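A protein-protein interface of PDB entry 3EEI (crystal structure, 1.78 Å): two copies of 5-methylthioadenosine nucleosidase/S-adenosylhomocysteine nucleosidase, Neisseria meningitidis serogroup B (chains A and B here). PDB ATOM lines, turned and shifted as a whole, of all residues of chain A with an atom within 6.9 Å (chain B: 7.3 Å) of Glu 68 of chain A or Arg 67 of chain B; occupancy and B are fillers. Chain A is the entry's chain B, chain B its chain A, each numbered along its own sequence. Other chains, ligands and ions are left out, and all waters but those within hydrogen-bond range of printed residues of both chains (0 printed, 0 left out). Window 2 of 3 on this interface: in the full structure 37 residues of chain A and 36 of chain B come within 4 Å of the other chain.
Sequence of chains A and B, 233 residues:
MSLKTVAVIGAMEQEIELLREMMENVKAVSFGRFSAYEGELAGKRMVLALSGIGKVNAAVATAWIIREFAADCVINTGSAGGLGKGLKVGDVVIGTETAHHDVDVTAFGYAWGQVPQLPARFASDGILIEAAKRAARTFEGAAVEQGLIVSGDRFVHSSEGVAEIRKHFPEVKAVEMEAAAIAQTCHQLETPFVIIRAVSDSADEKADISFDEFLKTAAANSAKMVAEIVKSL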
ATOM      1  N   VAL A  29       9.315 -31.951  25.949  1.00  0.00           N
ATOM      2  CA  VAL A  29       9.685 -30.864  25.063  1.00  0.00           C
ATOM      3  C   VAL A  29      10.747 -30.057  25.760  1.00  0.00           C
ATOM      4  O   VAL A  29      10.873 -30.127  26.979  1.00  0.00           O
ATOM      5  CB  VAL A  29       8.471 -29.960  24.675  1.00  0.00           C
ATOM      6  CG1 VAL A  29       7.429 -30.781  23.886  1.00  0.00           C
ATOM      7  CG2 VAL A  29       7.846 -29.371  25.895  1.00  0.00           C
ATOM      8  N   SER A  30      11.540 -29.316  24.994  1.00  0.00           N
ATOM      9  CA  SER A  30      12.634 -28.566  25.621  1.00  0.00           C
ATOM     10  C   SER A  30      12.880 -27.246  24.941  1.00  0.00           C
ATOM     11  O   SER A  30      12.349 -26.978  23.858  1.00  0.00           O
ATOM     12  CB  SER A  30      13.906 -29.397  25.666  1.00  0.00           C
ATOM     13  OG  SER A  30      14.437 -29.611  24.365  1.00  0.00           O
ATOM     14  N   PHE A  31      13.665 -26.403  25.592  1.00  0.00           N
ATOM     15  CA  PHE A  31      14.013 -25.099  25.046  1.00  0.00           C
ATOM     16  C   PHE A  31      15.323 -24.870  25.763  1.00  0.00           C
ATOM     17  O   PHE A  31      15.327 -24.510  26.942  1.00  0.00           O
ATOM     18  CB  PHE A  31      12.975 -24.057  25.470  1.00  0.00           C
ATOM     19  CG  PHE A  31      13.295 -22.613  25.066  1.00  0.00           C
ATOM     20  CD1 PHE A  31      13.869 -22.318  23.844  1.00  0.00           C
ATOM     21  CD2 PHE A  31      12.965 -21.554  25.909  1.00  0.00           C
ATOM     22  CE1 PHE A  31      14.131 -20.996  23.461  1.00  0.00           C
ATOM     23  CE2 PHE A  31      13.221 -20.232  25.532  1.00  0.00           C
ATOM     24  CZ  PHE A  31      13.803 -19.958  24.312  1.00  0.00           C
ATOM     25  N   ARG A  45      -5.539 -29.749  27.558  1.00  0.00           N
ATOM     26  CA  ARG A  45      -4.169 -29.778  27.129  1.00  0.00           C
ATOM     27  C   ARG A  45      -3.368 -29.185  28.290  1.00  0.00           C
ATOM     28  O   ARG A  45      -3.688 -28.109  28.764  1.00  0.00           O
ATOM     29  CB  ARG A  45      -4.032 -28.913  25.895  1.00  0.00           C
ATOM     30  CG  ARG A  45      -2.870 -29.251  25.033  1.00  0.00           C
ATOM     31  CD  ARG A  45      -2.714 -28.251  23.875  1.00  0.00           C
ATOM     32  NE  ARG A  45      -1.456 -28.512  23.212  1.00  0.00           N
ATOM     33  CZ  ARG A  45      -0.621 -27.597  22.725  1.00  0.00           C
ATOM     34  NH1 ARG A  45       0.491 -28.015  22.155  1.00  0.00           N
ATOM     35  NH2 ARG A  45      -0.869 -26.282  22.802  1.00  0.00           N
ATOM     36  N   ALA A  63       7.555 -17.601  30.192  1.00  0.00           N
ATOM     37  CA  ALA A  63       7.416 -16.925  28.893  1.00  0.00           C
ATOM     38  C   ALA A  63       7.496 -17.918  27.726  1.00  0.00           C
ATOM     39  O   ALA A  63       6.764 -17.792  26.730  1.00  0.00           O
ATOM     40  CB  ALA A  63       8.483 -15.812  28.747  1.00  0.00           C
ATOM     41  N   TRP A  64       8.393 -18.893  27.838  1.00  0.00           N
ATOM     42  CA  TRP A  64       8.562 -19.940  26.801  1.00  0.00           C
ATOM     43  C   TRP A  64       7.274 -20.715  26.602  1.00  0.00           C
ATOM     44  O   TRP A  64       6.805 -20.901  25.454  1.00  0.00           O
ATOM     45  CB  TRP A  64       9.689 -20.911  27.173  1.00  0.00           C
ATOM     46  CG  TRP A  64       9.638 -22.247  26.425  1.00  0.00           C
ATOM     47  CD1 TRP A  64       9.380 -22.433  25.114  1.00  0.00           C
ATOM     48  CD2 TRP A  64       9.868 -23.558  26.979  1.00  0.00           C
ATOM     49  NE1 TRP A  64       9.398 -23.778  24.811  1.00  0.00           N
ATOM     50  CE2 TRP A  64       9.710 -24.484  25.941  1.00  0.00           C
ATOM     51  CE3 TRP A  64      10.209 -24.025  28.257  1.00  0.00           C
ATOM     52  CZ2 TRP A  64       9.879 -25.857  26.130  1.00  0.00           C
ATOM     53  CZ3 TRP A  64      10.381 -25.369  28.437  1.00  0.00           C
ATOM     54  CH2 TRP A  64      10.206 -26.279  27.378  1.00  0.00           C
ATOM     55  N   ILE A  65       6.674 -21.170  27.704  1.00  0.00           N
ATOM     56  CA  ILE A  65       5.456 -21.971  27.571  1.00  0.00           C
ATOM     57  C   ILE A  65       4.297 -21.125  27.038  1.00  0.00           C
ATOM     58  O   ILE A  65       3.536 -21.554  26.185  1.00  0.00           O
ATOM     59  CB  ILE A  65       5.043 -22.637  28.877  1.00  0.00           C
ATOM     60  CG1 ILE A  65       6.158 -23.558  29.367  1.00  0.00           C
ATOM     61  CG2 ILE A  65       3.816 -23.511  28.644  1.00  0.00           C
ATOM     62  CD1 ILE A  65       6.673 -24.549  28.332  1.00  0.00           C
ATOM     63  N   ILE A  66       4.168 -19.905  27.518  1.00  0.00           N
ATOM     64  CA  ILE A  66       3.146 -19.017  26.938  1.00  0.00           C
ATOM     65  C   ILE A  66       3.332 -18.870  25.425  1.00  0.00           C
ATOM     66  O   ILE A  66       2.377 -19.010  24.670  1.00  0.00           O
ATOM     67  CB  ILE A  66       3.134 -17.659  27.629  1.00  0.00           C
ATOM     68  CG1 ILE A  66       2.584 -17.820  29.057  1.00  0.00           C
ATOM     69  CG2 ILE A  66       2.285 -16.646  26.839  1.00  0.00           C
ATOM     70  CD1 ILE A  66       2.726 -16.575  29.927  1.00  0.00           C
ATOM     71  N   ARG A  67       4.549 -18.553  24.989  1.00  0.00           N
ATOM     72  CA  ARG A  67       4.830 -18.257  23.588  1.00  0.00           C
ATOM     73  C   ARG A  67       4.704 -19.471  22.680  1.00  0.00           C
ATOM     74  O   ARG A  67       4.084 -19.400  21.612  1.00  0.00           O
ATOM     75  CB  ARG A  67       6.243 -17.665  23.461  1.00  0.00           C
ATOM     76  CG  ARG A  67       6.769 -17.530  22.024  1.00  0.00           C
ATOM     77  CD  ARG A  67       5.796 -16.738  21.199  1.00  0.00           C
ATOM     78  NE  ARG A  67       6.271 -16.551  19.825  1.00  0.00           N
ATOM     79  CZ  ARG A  67       6.091 -17.431  18.846  1.00  0.00           C
ATOM     80  NH1 ARG A  67       5.460 -18.589  19.070  1.00  0.00           N
ATOM     81  NH2 ARG A  67       6.564 -17.155  17.637  1.00  0.00           N
ATOM     82  N   GLU A  68       5.326 -20.574  23.086  1.00  0.00           N
ATOM     83  CA  GLU A  68       5.430 -21.725  22.223  1.00  0.00           C
ATOM     84  C   GLU A  68       4.143 -22.559  22.203  1.00  0.00           C
ATOM     85  O   GLU A  68       3.791 -23.114  21.177  1.00  0.00           O
ATOM     86  CB  GLU A  68       6.558 -22.621  22.661  1.00  0.00           C
ATOM     87  CG  GLU A  68       6.390 -23.973  22.062  1.00  0.00           C
ATOM     88  CD  GLU A  68       7.618 -24.484  21.405  1.00  0.00           C
ATOM     89  OE1 GLU A  68       8.644 -24.676  22.106  1.00  0.00           O
ATOM     90  OE2 GLU A  68       7.562 -24.713  20.174  1.00  0.00           O
ATOM     91  N   PHE A  69       3.458 -22.651  23.342  1.00  0.00           N
ATOM     92  CA  PHE A  69       2.263 -23.457  23.423  1.00  0.00           C
ATOM     93  C   PHE A  69       0.942 -22.690  23.502  1.00  0.00           C
ATOM     94  O   PHE A  69      -0.105 -23.317  23.585  1.00  0.00           O
ATOM     95  CB  PHE A  69       2.401 -24.467  24.571  1.00  0.00           C
ATOM     96  CG  PHE A  69       3.579 -25.388  24.390  1.00  0.00           C
ATOM     97  CD1 PHE A  69       3.500 -26.484  23.541  1.00  0.00           C
ATOM     98  CD2 PHE A  69       4.780 -25.122  25.028  1.00  0.00           C
ATOM     99  CE1 PHE A  69       4.583 -27.314  23.326  1.00  0.00           C
ATOM    100  CE2 PHE A  69       5.866 -25.947  24.850  1.00  0.00           C
ATOM    101  CZ  PHE A  69       5.787 -27.053  23.971  1.00  0.00           C
ATOM    102  N   ALA A  70       0.975 -21.368  23.479  1.00  0.00           N
ATOM    103  CA  ALA A  70      -0.252 -20.589  23.484  1.00  0.00           C
ATOM    104  C   ALA A  70      -1.080 -20.949  24.726  1.00  0.00           C
ATOM    105  O   ALA A  70      -2.278 -21.159  24.659  1.00  0.00           O
ATOM    106  CB  ALA A  70      -1.064 -20.827  22.186  1.00  0.00           C
ATOM    107  N   ALA A  71      -0.426 -20.981  25.881  1.00  0.00           N
ATOM    108  CA  ALA A  71      -1.117 -21.398  27.081  1.00  0.00           C
ATOM    109  C   ALA A  71      -2.210 -20.382  27.400  1.00  0.00           C
ATOM    110  O   ALA A  71      -1.980 -19.171  27.311  1.00  0.00           O
ATOM    111  CB  ALA A  71      -0.124 -21.537  28.244  1.00  0.00           C
ATOM    112  N   PHE B  31       5.848  -8.574  21.718  1.00  0.00           N
ATOM    113  CA  PHE B  31       5.448  -9.854  22.303  1.00  0.00           C
ATOM    114  C   PHE B  31       4.777  -9.422  23.577  1.00  0.00           C
ATOM    115  O   PHE B  31       5.475  -8.970  24.487  1.00  0.00           O
ATOM    116  CB  PHE B  31       6.704 -10.655  22.634  1.00  0.00           C
ATOM    117  CG  PHE B  31       6.453 -11.929  23.407  1.00  0.00           C
ATOM    118  CD1 PHE B  31       5.311 -12.676  23.191  1.00  0.00           C
ATOM    119  CD2 PHE B  31       7.395 -12.395  24.310  1.00  0.00           C
ATOM    120  CE1 PHE B  31       5.080 -13.866  23.888  1.00  0.00           C
ATOM    121  CE2 PHE B  31       7.167 -13.593  25.012  1.00  0.00           C
ATOM    122  CZ  PHE B  31       6.000 -14.317  24.783  1.00  0.00           C
ATOM    123  N   ALA B  61      12.536 -10.682  28.000  1.00  0.00           N
ATOM    124  CA  ALA B  61      12.854 -10.043  26.726  1.00  0.00           C
ATOM    125  C   ALA B  61      13.943 -10.802  25.991  1.00  0.00           C
ATOM    126  O   ALA B  61      13.866 -11.017  24.788  1.00  0.00           O
ATOM    127  CB  ALA B  61      13.274  -8.591  26.977  1.00  0.00           C
ATOM    128  N   THR B  62      14.979 -11.203  26.713  1.00  0.00           N
ATOM    129  CA  THR B  62      16.077 -11.949  26.144  1.00  0.00           C
ATOM    130  C   THR B  62      15.618 -13.310  25.616  1.00  0.00           C
ATOM    131  O   THR B  62      16.083 -13.755  24.561  1.00  0.00           O
ATOM    132  CB  THR B  62      17.178 -12.177  27.190  1.00  0.00           C
ATOM    133  OG1 THR B  62      17.667 -10.909  27.634  1.00  0.00           O
ATOM    134  CG2 THR B  62      18.369 -12.938  26.595  1.00  0.00           C
ATOM    135  N   ALA B  63      14.745 -13.977  26.368  1.00  0.00           N
ATOM    136  CA  ALA B  63      14.303 -15.321  25.948  1.00  0.00           C
ATOM    137  C   ALA B  63      13.470 -15.169  24.671  1.00  0.00           C
ATOM    138  O   ALA B  63      13.589 -15.951  23.718  1.00  0.00           O
ATOM    139  CB  ALA B  63      13.461 -15.950  27.044  1.00  0.00           C
ATOM    140  N   TRP B  64      12.627 -14.137  24.662  1.00  0.00           N
ATOM    141  CA  TRP B  64      11.839 -13.834  23.478  1.00  0.00           C
ATOM    142  C   TRP B  64      12.691 -13.614  22.239  1.00  0.00           C
ATOM    143  O   TRP B  64      12.446 -14.241  21.204  1.00  0.00           O
ATOM    144  CB  TRP B  64      10.965 -12.637  23.736  1.00  0.00           C
ATOM    145  CG  TRP B  64      10.312 -12.105  22.518  1.00  0.00           C
ATOM    146  CD1 TRP B  64       9.709 -12.816  21.528  1.00  0.00           C
ATOM    147  CD2 TRP B  64      10.169 -10.717  22.174  1.00  0.00           C
ATOM    148  NE1 TRP B  64       9.192 -11.943  20.571  1.00  0.00           N
ATOM    149  CE2 TRP B  64       9.475 -10.657  20.944  1.00  0.00           C
ATOM    150  CE3 TRP B  64      10.558  -9.524  22.794  1.00  0.00           C
ATOM    151  CZ2 TRP B  64       9.175  -9.463  20.319  1.00  0.00           C
ATOM    152  CZ3 TRP B  64      10.252  -8.319  22.159  1.00  0.00           C
ATOM    153  CH2 TRP B  64       9.575  -8.310  20.936  1.00  0.00           C
ATOM    154  N   ILE B  65      13.687 -12.735  22.305  1.00  0.00           N
ATOM    155  CA  ILE B  65      14.453 -12.470  21.096  1.00  0.00           C
ATOM    156  C   ILE B  65      15.223 -13.698  20.650  1.00  0.00           C
ATOM    157  O   ILE B  65      15.387 -13.940  19.464  1.00  0.00           O
ATOM    158  CB  ILE B  65      15.437 -11.315  21.250  1.00  0.00           C
ATOM    159  CG1 ILE B  65      14.684 -10.058  21.708  1.00  0.00           C
ATOM    160  CG2 ILE B  65      16.196 -11.140  19.932  1.00  0.00           C
ATOM    161  CD1 ILE B  65      13.595  -9.614  20.779  1.00  0.00           C
ATOM    162  N   ILE B  66      15.721 -14.473  21.597  1.00  0.00           N
ATOM    163  CA  ILE B  66      16.445 -15.659  21.213  1.00  0.00           C
ATOM    164  C   ILE B  66      15.505 -16.603  20.476  1.00  0.00           C
ATOM    165  O   ILE B  66      15.834 -17.059  19.381  1.00  0.00           O
ATOM    166  CB  ILE B  66      17.071 -16.369  22.416  1.00  0.00           C
ATOM    167  CG1 ILE B  66      18.280 -15.579  22.896  1.00  0.00           C
ATOM    168  CG2 ILE B  66      17.450 -17.846  22.068  1.00  0.00           C
ATOM    169  CD1 ILE B  66      18.788 -16.010  24.263  1.00  0.00           C
ATOM    170  N   ARG B  67      14.334 -16.855  21.049  1.00  0.00           N
ATOM    171  CA  ARG B  67      13.350 -17.779  20.480  1.00  0.00           C
ATOM    172  C   ARG B  67      12.904 -17.288  19.120  1.00  0.00           C
ATOM    173  O   ARG B  67      13.041 -17.967  18.101  1.00  0.00           O
ATOM    174  CB  ARG B  67      12.104 -17.816  21.369  1.00  0.00           C
ATOM    175  CG  ARG B  67      10.960 -18.739  20.904  1.00  0.00           C
ATOM    176  CD  ARG B  67      11.243 -20.099  21.479  1.00  0.00           C
ATOM    177  NE  ARG B  67      10.329 -21.191  21.139  1.00  0.00           N
ATOM    178  CZ  ARG B  67       9.291 -21.135  20.309  1.00  0.00           C
ATOM    179  NH1 ARG B  67       8.949 -20.011  19.719  1.00  0.00           N
ATOM    180  NH2 ARG B  67       8.578 -22.238  20.091  1.00  0.00           N
ATOM    181  N   GLU B  68      12.334 -16.099  19.147  1.00  0.00           N
ATOM    182  CA  GLU B  68      11.635 -15.511  18.035  1.00  0.00           C
ATOM    183  C   GLU B  68      12.551 -15.245  16.824  1.00  0.00           C
ATOM    184  O   GLU B  68      12.121 -15.392  15.677  1.00  0.00           O
ATOM    185  CB  GLU B  68      10.977 -14.223  18.525  1.00  0.00           C
ATOM    186  CG  GLU B  68       9.973 -13.615  17.577  1.00  0.00           C
ATOM    187  CD  GLU B  68       8.619 -14.314  17.642  1.00  0.00           C
ATOM    188  OE1 GLU B  68       8.013 -14.384  18.750  1.00  0.00           O
ATOM    189  OE2 GLU B  68       8.163 -14.780  16.573  1.00  0.00           O
ATOM    190  N   PHE B  69      13.803 -14.866  17.067  1.00  0.00           N
ATOM    191  CA  PHE B  69      14.684 -14.466  15.979  1.00  0.00           C
ATOM    192  C   PHE B  69      15.916 -15.332  15.833  1.00  0.00           C
ATOM    193  O   PHE B  69      16.769 -15.059  15.001  1.00  0.00           O
ATOM    194  CB  PHE B  69      15.087 -13.003  16.141  1.00  0.00           C
ATOM    195  CG  PHE B  69      13.931 -12.070  16.138  1.00  0.00           C
ATOM    196  CD1 PHE B  69      13.371 -11.653  14.948  1.00  0.00           C
ATOM    197  CD2 PHE B  69      13.387 -11.613  17.312  1.00  0.00           C
ATOM    198  CE1 PHE B  69      12.274 -10.807  14.952  1.00  0.00           C
ATOM    199  CE2 PHE B  69      12.314 -10.766  17.310  1.00  0.00           C
ATOM    200  CZ  PHE B  69      11.758 -10.364  16.127  1.00  0.00           C
ATOM    201  N   ALA B  70      16.034 -16.384  16.624  1.00  0.00           N
ATOM    202  CA  ALA B  70      17.184 -17.259  16.479  1.00  0.00           C
ATOM    203  C   ALA B  70      18.464 -16.436  16.597  1.00  0.00           C
ATOM    204  O   ALA B  70      19.419 -16.633  15.830  1.00  0.00           O
ATOM    205  CB  ALA B  70      17.147 -17.957  15.112  1.00  0.00           C
ATOM    206  N   ALA B  71      18.488 -15.498  17.540  1.00  0.00           N
ATOM    207  CA  ALA B  71      19.666 -14.671  17.706  1.00  0.00           C
ATOM    208  C   ALA B  71      20.922 -15.518  17.905  1.00  0.00           C
ATOM    209  O   ALA B  71      20.933 -16.437  18.720  1.00  0.00           O
ATOM    210  CB  ALA B  71      19.475 -13.735  18.867  1.00  0.00           C
ATOM    211  N   LEU B 189      19.996 -20.918  27.593  1.00  0.00           N
ATOM    212  CA  LEU B 189      19.570 -21.073  26.201  1.00  0.00           C
ATOM    213  C   LEU B 189      20.789 -21.221  25.292  1.00  0.00           C
ATOM    214  O   LEU B 189      20.701 -21.031  24.076  1.00  0.00           O
ATOM    215  CB  LEU B 189      18.729 -19.876  25.778  1.00  0.00           C
ATOM    216  CG  LEU B 189      17.420 -19.725  26.593  1.00  0.00           C
ATOM    217  CD1 LEU B 189      16.506 -18.525  26.157  1.00  0.00           C
ATOM    218  CD2 LEU B 189      16.652 -21.038  26.579  1.00  0.00           C
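Of the printed residues of chain B, Phe 31 of chain A touches Arg 67 (3.6 Å) and Leu 189 (3.6 Å).
Arg 45 of chain A touches none of the printed residues of chain B.
Ile 65 of chain A touches none of the printed residues of chain B.
Of chain B, only Arg 67 comes within 4 Å of Glu 68 of chain A.
Of the printed residues of chain A, Phe 31 of chain B touches Arg 67 (3.6 Å).
Arg 67 of chain B touches just these residues of chain A: Phe 31 (3.6 Å), Arg 67 (3.8 Å) and Glu 68 (2.7 Å).
Printed residues of chain A within 4 Å of Glu 68 of chain B: Arg 67 (3.0 Å).
Printed residues of chain A within 4 Å of Leu 189 of chain B: Phe 31.
The nearest residue of chain B that does not touch Glu 68 of chain A is Phe 31 of chain B (6.5 Å).
Among the printed residues, merely in contact across the chains: Phe 31 of chain A with Leu 189 of chain B, Arg 67 of chain A with Phe 31 of chain B, Phe 31 of chain A with Arg 67 of chain B and Arg 67 of chain A with Arg 67 of chain B.
OE1 of Glu 68 of chain B is in hydrogen-bond range of NE1 of Trp 64 of chain B (3.3 Å).
The indole nitrogen of Trp 64 of chain A sits at hydrogen-bond distance from the side-chain carboxylate of Glu 68 of chain A.
Hydrophobic or aromatic side chains of chain B within 4 Å of the printed part of chain A: Phe 31 and Leu 189.
Printed residues of chain A that touch a printed residue of chain B: Phe 31, Arg 67 and Glu 68.
The guanidinium group (NH2) of Arg 67 of chain B lies within salt-bridge range of the side-chain carboxylate (OE2) of Glu 68 of chain A (2.7 Å).
The guanidinium group (NE) of Arg 67 of chain A is in salt-bridge range of the side-chain carboxylate (OE1) of Glu 68 of chain B, 3.0 Å away.
Phe 31 of chain A touches Arg 67 of chain B, and with the chains exchanged Arg 67 of chain A touches Phe 31 of chain B.
Arg 67 of chain B touches its own counterpart, Arg 67 of chain A.
Arg 67 of chain A touches Glu 68 of chain B, and with the chains exchanged Glu 68 of chain A touches Arg 67 of chain B.
Of the 6 pairs that touch across the chains among the printed residues, 5 have their exchanged pair printed and touching as well.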
